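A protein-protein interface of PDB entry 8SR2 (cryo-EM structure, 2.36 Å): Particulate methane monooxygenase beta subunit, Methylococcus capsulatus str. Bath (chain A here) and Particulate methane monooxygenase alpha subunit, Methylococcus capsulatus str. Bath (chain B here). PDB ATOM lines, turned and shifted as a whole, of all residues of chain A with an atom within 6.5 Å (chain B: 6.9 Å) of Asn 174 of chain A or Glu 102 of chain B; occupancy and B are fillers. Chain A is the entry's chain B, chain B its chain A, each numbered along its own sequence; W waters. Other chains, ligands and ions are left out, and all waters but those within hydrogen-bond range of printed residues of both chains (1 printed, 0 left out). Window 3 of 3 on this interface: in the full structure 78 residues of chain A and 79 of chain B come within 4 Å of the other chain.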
ATOM      1  N   GLU A 172      19.964  14.733  15.969  1.00  0.00           N
ATOM      2  CA  GLU A 172      19.782  15.338  17.285  1.00  0.00           C
ATOM      3  C   GLU A 172      18.761  16.462  17.148  1.00  0.00           C
ATOM      4  O   GLU A 172      19.079  17.543  16.645  1.00  0.00           O
ATOM      5  CB  GLU A 172      21.110  15.864  17.823  1.00  0.00           C
ATOM      6  CG  GLU A 172      21.353  15.553  19.286  1.00  0.00           C
ATOM      7  CD  GLU A 172      20.312  16.175  20.191  1.00  0.00           C
ATOM      8  OE1 GLU A 172      20.040  17.385  20.048  1.00  0.00           O
ATOM      9  OE2 GLU A 172      19.767  15.450  21.049  1.00  0.00           O
ATOM     10  N   TYR A 173      17.532  16.208  17.593  1.00  0.00           N
ATOM     11  CA  TYR A 173      16.425  17.147  17.425  1.00  0.00           C
ATOM     12  C   TYR A 173      15.935  17.589  18.801  1.00  0.00           C
ATOM     13  O   TYR A 173      15.163  16.876  19.450  1.00  0.00           O
ATOM     14  CB  TYR A 173      15.299  16.519  16.609  1.00  0.00           C
ATOM     15  CG  TYR A 173      14.322  17.522  16.040  1.00  0.00           C
ATOM     16  CD1 TYR A 173      14.564  18.133  14.815  1.00  0.00           C
ATOM     17  CD2 TYR A 173      13.166  17.861  16.725  1.00  0.00           C
ATOM     18  CE1 TYR A 173      13.676  19.052  14.290  1.00  0.00           C
ATOM     19  CE2 TYR A 173      12.272  18.779  16.208  1.00  0.00           C
ATOM     20  CZ  TYR A 173      12.532  19.371  14.992  1.00  0.00           C
ATOM     21  OH  TYR A 173      11.646  20.286  14.472  1.00  0.00           O
ATOM     22  N   ASN A 174      16.366  18.781  19.209  1.00  0.00           N
ATOM     23  CA  ASN A 174      15.994  19.378  20.489  1.00  0.00           C
ATOM     24  C   ASN A 174      16.238  18.487  21.702  1.00  0.00           C
ATOM     25  O   ASN A 174      15.412  18.421  22.610  1.00  0.00           O
ATOM     26  CB  ASN A 174      14.540  19.864  20.464  1.00  0.00           C
ATOM     27  CG  ASN A 174      14.299  20.921  19.407  1.00  0.00           C
ATOM     28  OD1 ASN A 174      13.562  20.700  18.448  1.00  0.00           O
ATOM     29  ND2 ASN A 174      14.925  22.079  19.577  1.00  0.00           N
ATOM     30  N   GLY A 175      17.377  17.804  21.711  1.00  0.00           N
ATOM     31  CA  GLY A 175      17.735  16.938  22.818  1.00  0.00           C
ATOM     32  C   GLY A 175      17.248  15.507  22.694  1.00  0.00           C
ATOM     33  O   GLY A 175      17.681  14.636  23.443  1.00  0.00           O
ATOM     34  N   MET A 176      16.346  15.261  21.752  1.00  0.00           N
ATOM     35  CA  MET A 176      15.815  13.918  21.553  1.00  0.00           C
ATOM     36  C   MET A 176      16.315  13.309  20.251  1.00  0.00           C
ATOM     37  O   MET A 176      16.489  14.008  19.256  1.00  0.00           O
ATOM     38  CB  MET A 176      14.286  13.937  21.572  1.00  0.00           C
ATOM     39  CG  MET A 176      13.688  14.201  22.943  1.00  0.00           C
ATOM     40  SD  MET A 176      12.165  13.283  23.232  1.00  0.00           S
ATOM     41  CE  MET A 176      12.366  11.923  22.085  1.00  0.00           C
ATOM     42  N   TYR A 186       6.799  14.634  12.604  1.00  0.00           N
ATOM     43  CA  TYR A 186       6.638  15.603  13.675  1.00  0.00           C
ATOM     44  C   TYR A 186       6.342  16.983  13.096  1.00  0.00           C
ATOM     45  O   TYR A 186       5.484  17.704  13.600  1.00  0.00           O
ATOM     46  CB  TYR A 186       7.895  15.657  14.538  1.00  0.00           C
ATOM     47  CG  TYR A 186       7.753  16.524  15.765  1.00  0.00           C
ATOM     48  CD1 TYR A 186       6.675  16.369  16.623  1.00  0.00           C
ATOM     49  CD2 TYR A 186       8.695  17.496  16.063  1.00  0.00           C
ATOM     50  CE1 TYR A 186       6.539  17.160  17.747  1.00  0.00           C
ATOM     51  CE2 TYR A 186       8.568  18.290  17.185  1.00  0.00           C
ATOM     52  CZ  TYR A 186       7.488  18.117  18.022  1.00  0.00           C
ATOM     53  OH  TYR A 186       7.358  18.906  19.140  1.00  0.00           O
ATOM     54  N   ASN A 187       7.052  17.342  12.031  1.00  0.00           N
ATOM     55  CA  ASN A 187       6.875  18.638  11.386  1.00  0.00           C
ATOM     56  C   ASN A 187       5.538  18.768  10.665  1.00  0.00           C
ATOM     57  O   ASN A 187       4.612  19.393  11.173  1.00  0.00           O
ATOM     58  CB  ASN A 187       8.024  18.915  10.420  1.00  0.00           C
ATOM     59  CG  ASN A 187       9.323  19.217  11.135  1.00  0.00           C
ATOM     60  OD1 ASN A 187      10.383  19.283  10.516  1.00  0.00           O
ATOM     61  ND2 ASN A 187       9.246  19.405  12.444  1.00  0.00           N
ATOM     62  N   LEU B  89      -0.115  15.808  21.800  1.00  0.00           N
ATOM     63  CA  LEU B  89      -0.369  17.237  21.656  1.00  0.00           C
ATOM     64  C   LEU B  89      -0.263  17.596  20.180  1.00  0.00           C
ATOM     65  O   LEU B  89       0.833  17.775  19.647  1.00  0.00           O
ATOM     66  CB  LEU B  89       0.609  18.048  22.497  1.00  0.00           C
ATOM     67  CG  LEU B  89       0.468  19.570  22.429  1.00  0.00           C
ATOM     68  CD1 LEU B  89      -0.889  20.009  22.957  1.00  0.00           C
ATOM     69  CD2 LEU B  89       1.592  20.252  23.194  1.00  0.00           C
ATOM     70  N   VAL B  91      -1.892  19.864  16.616  1.00  0.00           N
ATOM     71  CA  VAL B  91      -2.284  21.215  16.227  1.00  0.00           C
ATOM     72  C   VAL B  91      -3.345  21.105  15.143  1.00  0.00           C
ATOM     73  O   VAL B  91      -3.169  20.367  14.168  1.00  0.00           O
ATOM     74  CB  VAL B  91      -1.083  22.041  15.727  1.00  0.00           C
ATOM     75  CG1 VAL B  91      -1.530  23.439  15.347  1.00  0.00           C
ATOM     76  CG2 VAL B  91       0.004  22.097  16.788  1.00  0.00           C
ATOM     77  N   ILE B  99       4.433  24.152  10.038  1.00  0.00           N
ATOM     78  CA  ILE B  99       5.163  22.956  10.441  1.00  0.00           C
ATOM     79  C   ILE B  99       5.432  23.051  11.936  1.00  0.00           C
ATOM     80  O   ILE B  99       5.864  24.098  12.430  1.00  0.00           O
ATOM     81  CB  ILE B  99       6.471  22.774   9.648  1.00  0.00           C
ATOM     82  CG1 ILE B  99       7.362  24.011   9.757  1.00  0.00           C
ATOM     83  CG2 ILE B  99       6.171  22.453   8.192  1.00  0.00           C
ATOM     84  CD1 ILE B  99       8.842  23.694   9.759  1.00  0.00           C
ATOM     85  N   ARG B 100       5.149  21.972  12.654  1.00  0.00           N
ATOM     86  CA  ARG B 100       5.361  21.949  14.092  1.00  0.00           C
ATOM     87  C   ARG B 100       6.845  21.867  14.407  1.00  0.00           C
ATOM     88  O   ARG B 100       7.427  20.786  14.424  1.00  0.00           O
ATOM     89  CB  ARG B 100       4.622  20.775  14.732  1.00  0.00           C
ATOM     90  CG  ARG B 100       4.663  20.779  16.249  1.00  0.00           C
ATOM     91  CD  ARG B 100       4.041  19.518  16.826  1.00  0.00           C
ATOM     92  NE  ARG B 100       3.863  18.488  15.809  1.00  0.00           N
ATOM     93  CZ  ARG B 100       2.739  17.806  15.629  1.00  0.00           C
ATOM     94  NH1 ARG B 100       1.687  18.046  16.398  1.00  0.00           N
ATOM     95  NH2 ARG B 100       2.665  16.887  14.679  1.00  0.00           N
ATOM     96  N   LYS B 101       7.457  23.020  14.647  1.00  0.00           N
ATOM     97  CA  LYS B 101       8.873  23.070  14.969  1.00  0.00           C
ATOM     98  C   LYS B 101       9.122  22.361  16.291  1.00  0.00           C
ATOM     99  O   LYS B 101       9.932  21.440  16.370  1.00  0.00           O
ATOM    100  CB  LYS B 101       9.348  24.520  15.052  1.00  0.00           C
ATOM    101  CG  LYS B 101      10.605  24.808  14.250  1.00  0.00           C
ATOM    102  CD  LYS B 101      10.822  23.764  13.168  1.00  0.00           C
ATOM    103  CE  LYS B 101      12.274  23.732  12.720  1.00  0.00           C
ATOM    104  NZ  LYS B 101      12.984  22.527  13.228  1.00  0.00           N
ATOM    105  N   GLU B 102       8.415  22.801  17.328  1.00  0.00           N
ATOM    106  CA  GLU B 102       8.542  22.227  18.664  1.00  0.00           C
ATOM    107  C   GLU B 102       7.204  22.230  19.398  1.00  0.00           C
ATOM    108  O   GLU B 102       6.316  23.024  19.093  1.00  0.00           O
ATOM    109  CB  GLU B 102       9.561  23.008  19.490  1.00  0.00           C
ATOM    110  CG  GLU B 102      11.009  22.798  19.082  1.00  0.00           C
ATOM    111  CD  GLU B 102      11.752  24.107  18.901  1.00  0.00           C
ATOM    112  OE1 GLU B 102      11.658  24.971  19.796  1.00  0.00           O
ATOM    113  OE2 GLU B 102      12.425  24.271  17.863  1.00  0.00           O
ATOM    114  N   SER B 103       7.070  21.334  20.369  1.00  0.00           N
ATOM    115  CA  SER B 103       5.860  21.224  21.175  1.00  0.00           C
ATOM    116  C   SER B 103       6.249  20.756  22.569  1.00  0.00           C
ATOM    117  O   SER B 103       6.983  19.783  22.714  1.00  0.00           O
ATOM    118  CB  SER B 103       4.870  20.248  20.541  1.00  0.00           C
ATOM    119  OG  SER B 103       5.478  18.996  20.290  1.00  0.00           O
ATOM    120  N   TYR B 104       5.761  21.445  23.595  1.00  0.00           N
ATOM    121  CA  TYR B 104       6.108  21.086  24.966  1.00  0.00           C
ATOM    122  C   TYR B 104       4.940  20.983  25.942  1.00  0.00           C
ATOM    123  O   TYR B 104       4.057  21.838  25.970  1.00  0.00           O
ATOM    124  CB  TYR B 104       7.097  22.103  25.548  1.00  0.00           C
ATOM    125  CG  TYR B 104       8.334  22.358  24.722  1.00  0.00           C
ATOM    126  CD1 TYR B 104       8.306  23.236  23.650  1.00  0.00           C
ATOM    127  CD2 TYR B 104       9.535  21.733  25.027  1.00  0.00           C
ATOM    128  CE1 TYR B 104       9.437  23.478  22.896  1.00  0.00           C
ATOM    129  CE2 TYR B 104      10.670  21.969  24.279  1.00  0.00           C
ATOM    130  CZ  TYR B 104      10.616  22.841  23.217  1.00  0.00           C
ATOM    131  OH  TYR B 104      11.744  23.080  22.469  1.00  0.00           O
ATOM    132  N   LEU B 109      10.220  18.648  25.768  1.00  0.00           N
ATOM    133  CA  LEU B 109       9.723  18.385  24.422  1.00  0.00           C
ATOM    134  C   LEU B 109       8.950  17.073  24.353  1.00  0.00           C
ATOM    135  O   LEU B 109       9.329  16.090  24.985  1.00  0.00           O
ATOM    136  CB  LEU B 109      10.883  18.361  23.425  1.00  0.00           C
ATOM    137  CG  LEU B 109      10.504  18.269  21.947  1.00  0.00           C
ATOM    138  CD1 LEU B 109      10.579  19.637  21.289  1.00  0.00           C
ATOM    139  CD2 LEU B 109      11.397  17.274  21.225  1.00  0.00           C
ATOM    140  N   VAL B 110       7.871  17.060  23.578  1.00  0.00           N
ATOM    141  CA  VAL B 110       7.049  15.864  23.443  1.00  0.00           C
ATOM    142  C   VAL B 110       6.722  15.544  21.990  1.00  0.00           C
ATOM    143  O   VAL B 110       5.639  15.866  21.510  1.00  0.00           O
ATOM    144  CB  VAL B 110       5.729  15.999  24.222  1.00  0.00           C
ATOM    145  CG1 VAL B 110       5.999  16.064  25.715  1.00  0.00           C
ATOM    146  CG2 VAL B 110       4.968  17.230  23.759  1.00  0.00           C
ATOM    147  N   ARG B 125       3.385  24.523  25.174  1.00  0.00           N
ATOM    148  CA  ARG B 125       3.988  25.525  24.300  1.00  0.00           C
ATOM    149  C   ARG B 125       4.267  24.872  22.957  1.00  0.00           C
ATOM    150  O   ARG B 125       5.016  23.892  22.889  1.00  0.00           O
ATOM    151  CB  ARG B 125       5.269  26.087  24.912  1.00  0.00           C
ATOM    152  CG  ARG B 125       5.979  27.106  24.039  1.00  0.00           C
ATOM    153  CD  ARG B 125       7.015  27.880  24.833  1.00  0.00           C
ATOM    154  NE  ARG B 125       8.301  27.195  24.870  1.00  0.00           N
ATOM    155  CZ  ARG B 125       9.240  27.311  23.940  1.00  0.00           C
ATOM    156  NH1 ARG B 125       9.070  28.084  22.878  1.00  0.00           N
ATOM    157  NH2 ARG B 125      10.376  26.636  24.077  1.00  0.00           N
ATOM    158  N   VAL B 126       3.668  25.407  21.896  1.00  0.00           N
ATOM    159  CA  VAL B 126       3.824  24.883  20.544  1.00  0.00           C
ATOM    160  C   VAL B 126       4.437  25.972  19.676  1.00  0.00           C
ATOM    161  O   VAL B 126       3.963  27.114  19.675  1.00  0.00           O
ATOM    162  CB  VAL B 126       2.482  24.409  19.960  1.00  0.00           C
ATOM    163  CG1 VAL B 126       2.680  23.867  18.555  1.00  0.00           C
ATOM    164  CG2 VAL B 126       1.853  23.356  20.859  1.00  0.00           C
ATOM    165  N   VAL B 127       5.488  25.618  18.942  1.00  0.00           N
ATOM    166  CA  VAL B 127       6.177  26.539  18.042  1.00  0.00           C
ATOM    167  C   VAL B 127       5.883  26.108  16.612  1.00  0.00           C
ATOM    168  O   VAL B 127       6.127  24.953  16.242  1.00  0.00           O
ATOM    169  CB  VAL B 127       7.690  26.567  18.311  1.00  0.00           C
ATOM    170  CG1 VAL B 127       8.371  27.568  17.393  1.00  0.00           C
ATOM    171  CG2 VAL B 127       7.962  26.898  19.770  1.00  0.00           C
ATOM    172  N   LEU B 128       5.360  27.034  15.815  1.00  0.00           N
ATOM    173  CA  LEU B 128       4.980  26.766  14.436  1.00  0.00           C
ATOM    174  C   LEU B 128       5.738  27.692  13.499  1.00  0.00           C
ATOM    175  O   LEU B 128       5.913  28.880  13.787  1.00  0.00           O
ATOM    176  CB  LEU B 128       3.471  26.943  14.232  1.00  0.00           C
ATOM    177  CG  LEU B 128       2.550  26.091  15.105  1.00  0.00           C
ATOM    178  CD1 LEU B 128       1.096  26.414  14.813  1.00  0.00           C
ATOM    179  CD2 LEU B 128       2.825  24.613  14.889  1.00  0.00           C
HETATM  180  O   HOH W   1      12.658  20.426  11.219  1.00  0.00           O
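O of Tyr 186 of chain A sits at hydrogen-bond distance from NE of Arg 100 of chain B (2.8 Å). N of Arg 100 of chain B lies within hydrogen-bond range of O of Asn 187 of chain A, 3.0 Å away. The side-chain hydroxyl of Tyr 173 of chain A sits at hydrogen-bond distance from the backbone carbonyl oxygen of Lys 101 of chain B. The backbone NH of Ser 103 of chain B lies within hydrogen-bond range of the side-chain hydroxyl of Tyr 186 of chain A (2.7 Å).
NH1 of Arg 100 of chain B is in hydrogen-bond range of O of Leu 89 of chain B (3.4 Å). The backbone NH (N) of Lys 101 of chain B lies within hydrogen-bond range of the backbone carbonyl oxygen (O) of Val 127 of chain B. OE1 of Glu 102 of chain B lies within hydrogen-bond range of OH of Tyr 104 of chain B (3.3 Å). The backbone carbonyl oxygen of Glu 102 of chain B lies within hydrogen-bond range of the backbone NH of Val 127 of chain B (2.7 Å). The backbone carbonyl oxygen (O) of Ser 103 of chain B sits at hydrogen-bond distance from the backbone NH (N) of Val 110 of chain B. The side-chain amide nitrogen (ND2) of Asn 187 of chain A is in hydrogen-bond range of the side-chain hydroxyl (OH) of Tyr 173 of chain A (3.3 Å).
Among the printed residues, merely in contact across the chains: Asn 174 of chain A with Glu 102 of chain B (3.4 Å), Tyr 186 of chain A with Lys 101 of chain B (3.5 Å), Tyr 186 of chain A with Glu 102 of chain B (3.3 Å), Tyr 186 of chain A with Leu 109 of chain B (3.9 Å) and Asn 187 of chain A with Ile 99 of chain B (3.7 Å).
Printed residues of chain B within 4 Å of Asn 174 of chain A: Glu 102. Of chain A, only Asn 174 (3.4 Å) and Tyr 186 (3.3 Å) come within 4 Å of Glu 102 of chain B. Of the printed residues of chain A, Arg 100 of chain B touches Tyr 186 (2.8 Å) and Asn 187 (3.0 Å). Of the printed residues of chain A, Leu 109 of chain B touches Tyr 186 (3.9 Å). The nearest residue of chain A that does not touch Glu 102 of chain B is Tyr 173 of chain A (5.0 Å). The nearest printed residue of chain A that does not touch Lys 101 of chain B is Asn 174 of chain A (4.2 Å).
Of the 14 printed residues of chain B, 6 touch a printed residue of chain A. Hydrophobic or aromatic side chains of chain B that line the printed part of chain A: Leu 109. Among the printed residues, 9 pairs touch across the chains.
Water W1 lies within hydrogen-bond range of the side-chain amide oxygen of Asn 187 of chain A (2.6 Å), the side-chain amino group of Lys 101 of chain B (2.9 Å) and the side-chain hydroxyl of Tyr 173 of chain A (3.4 Å).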
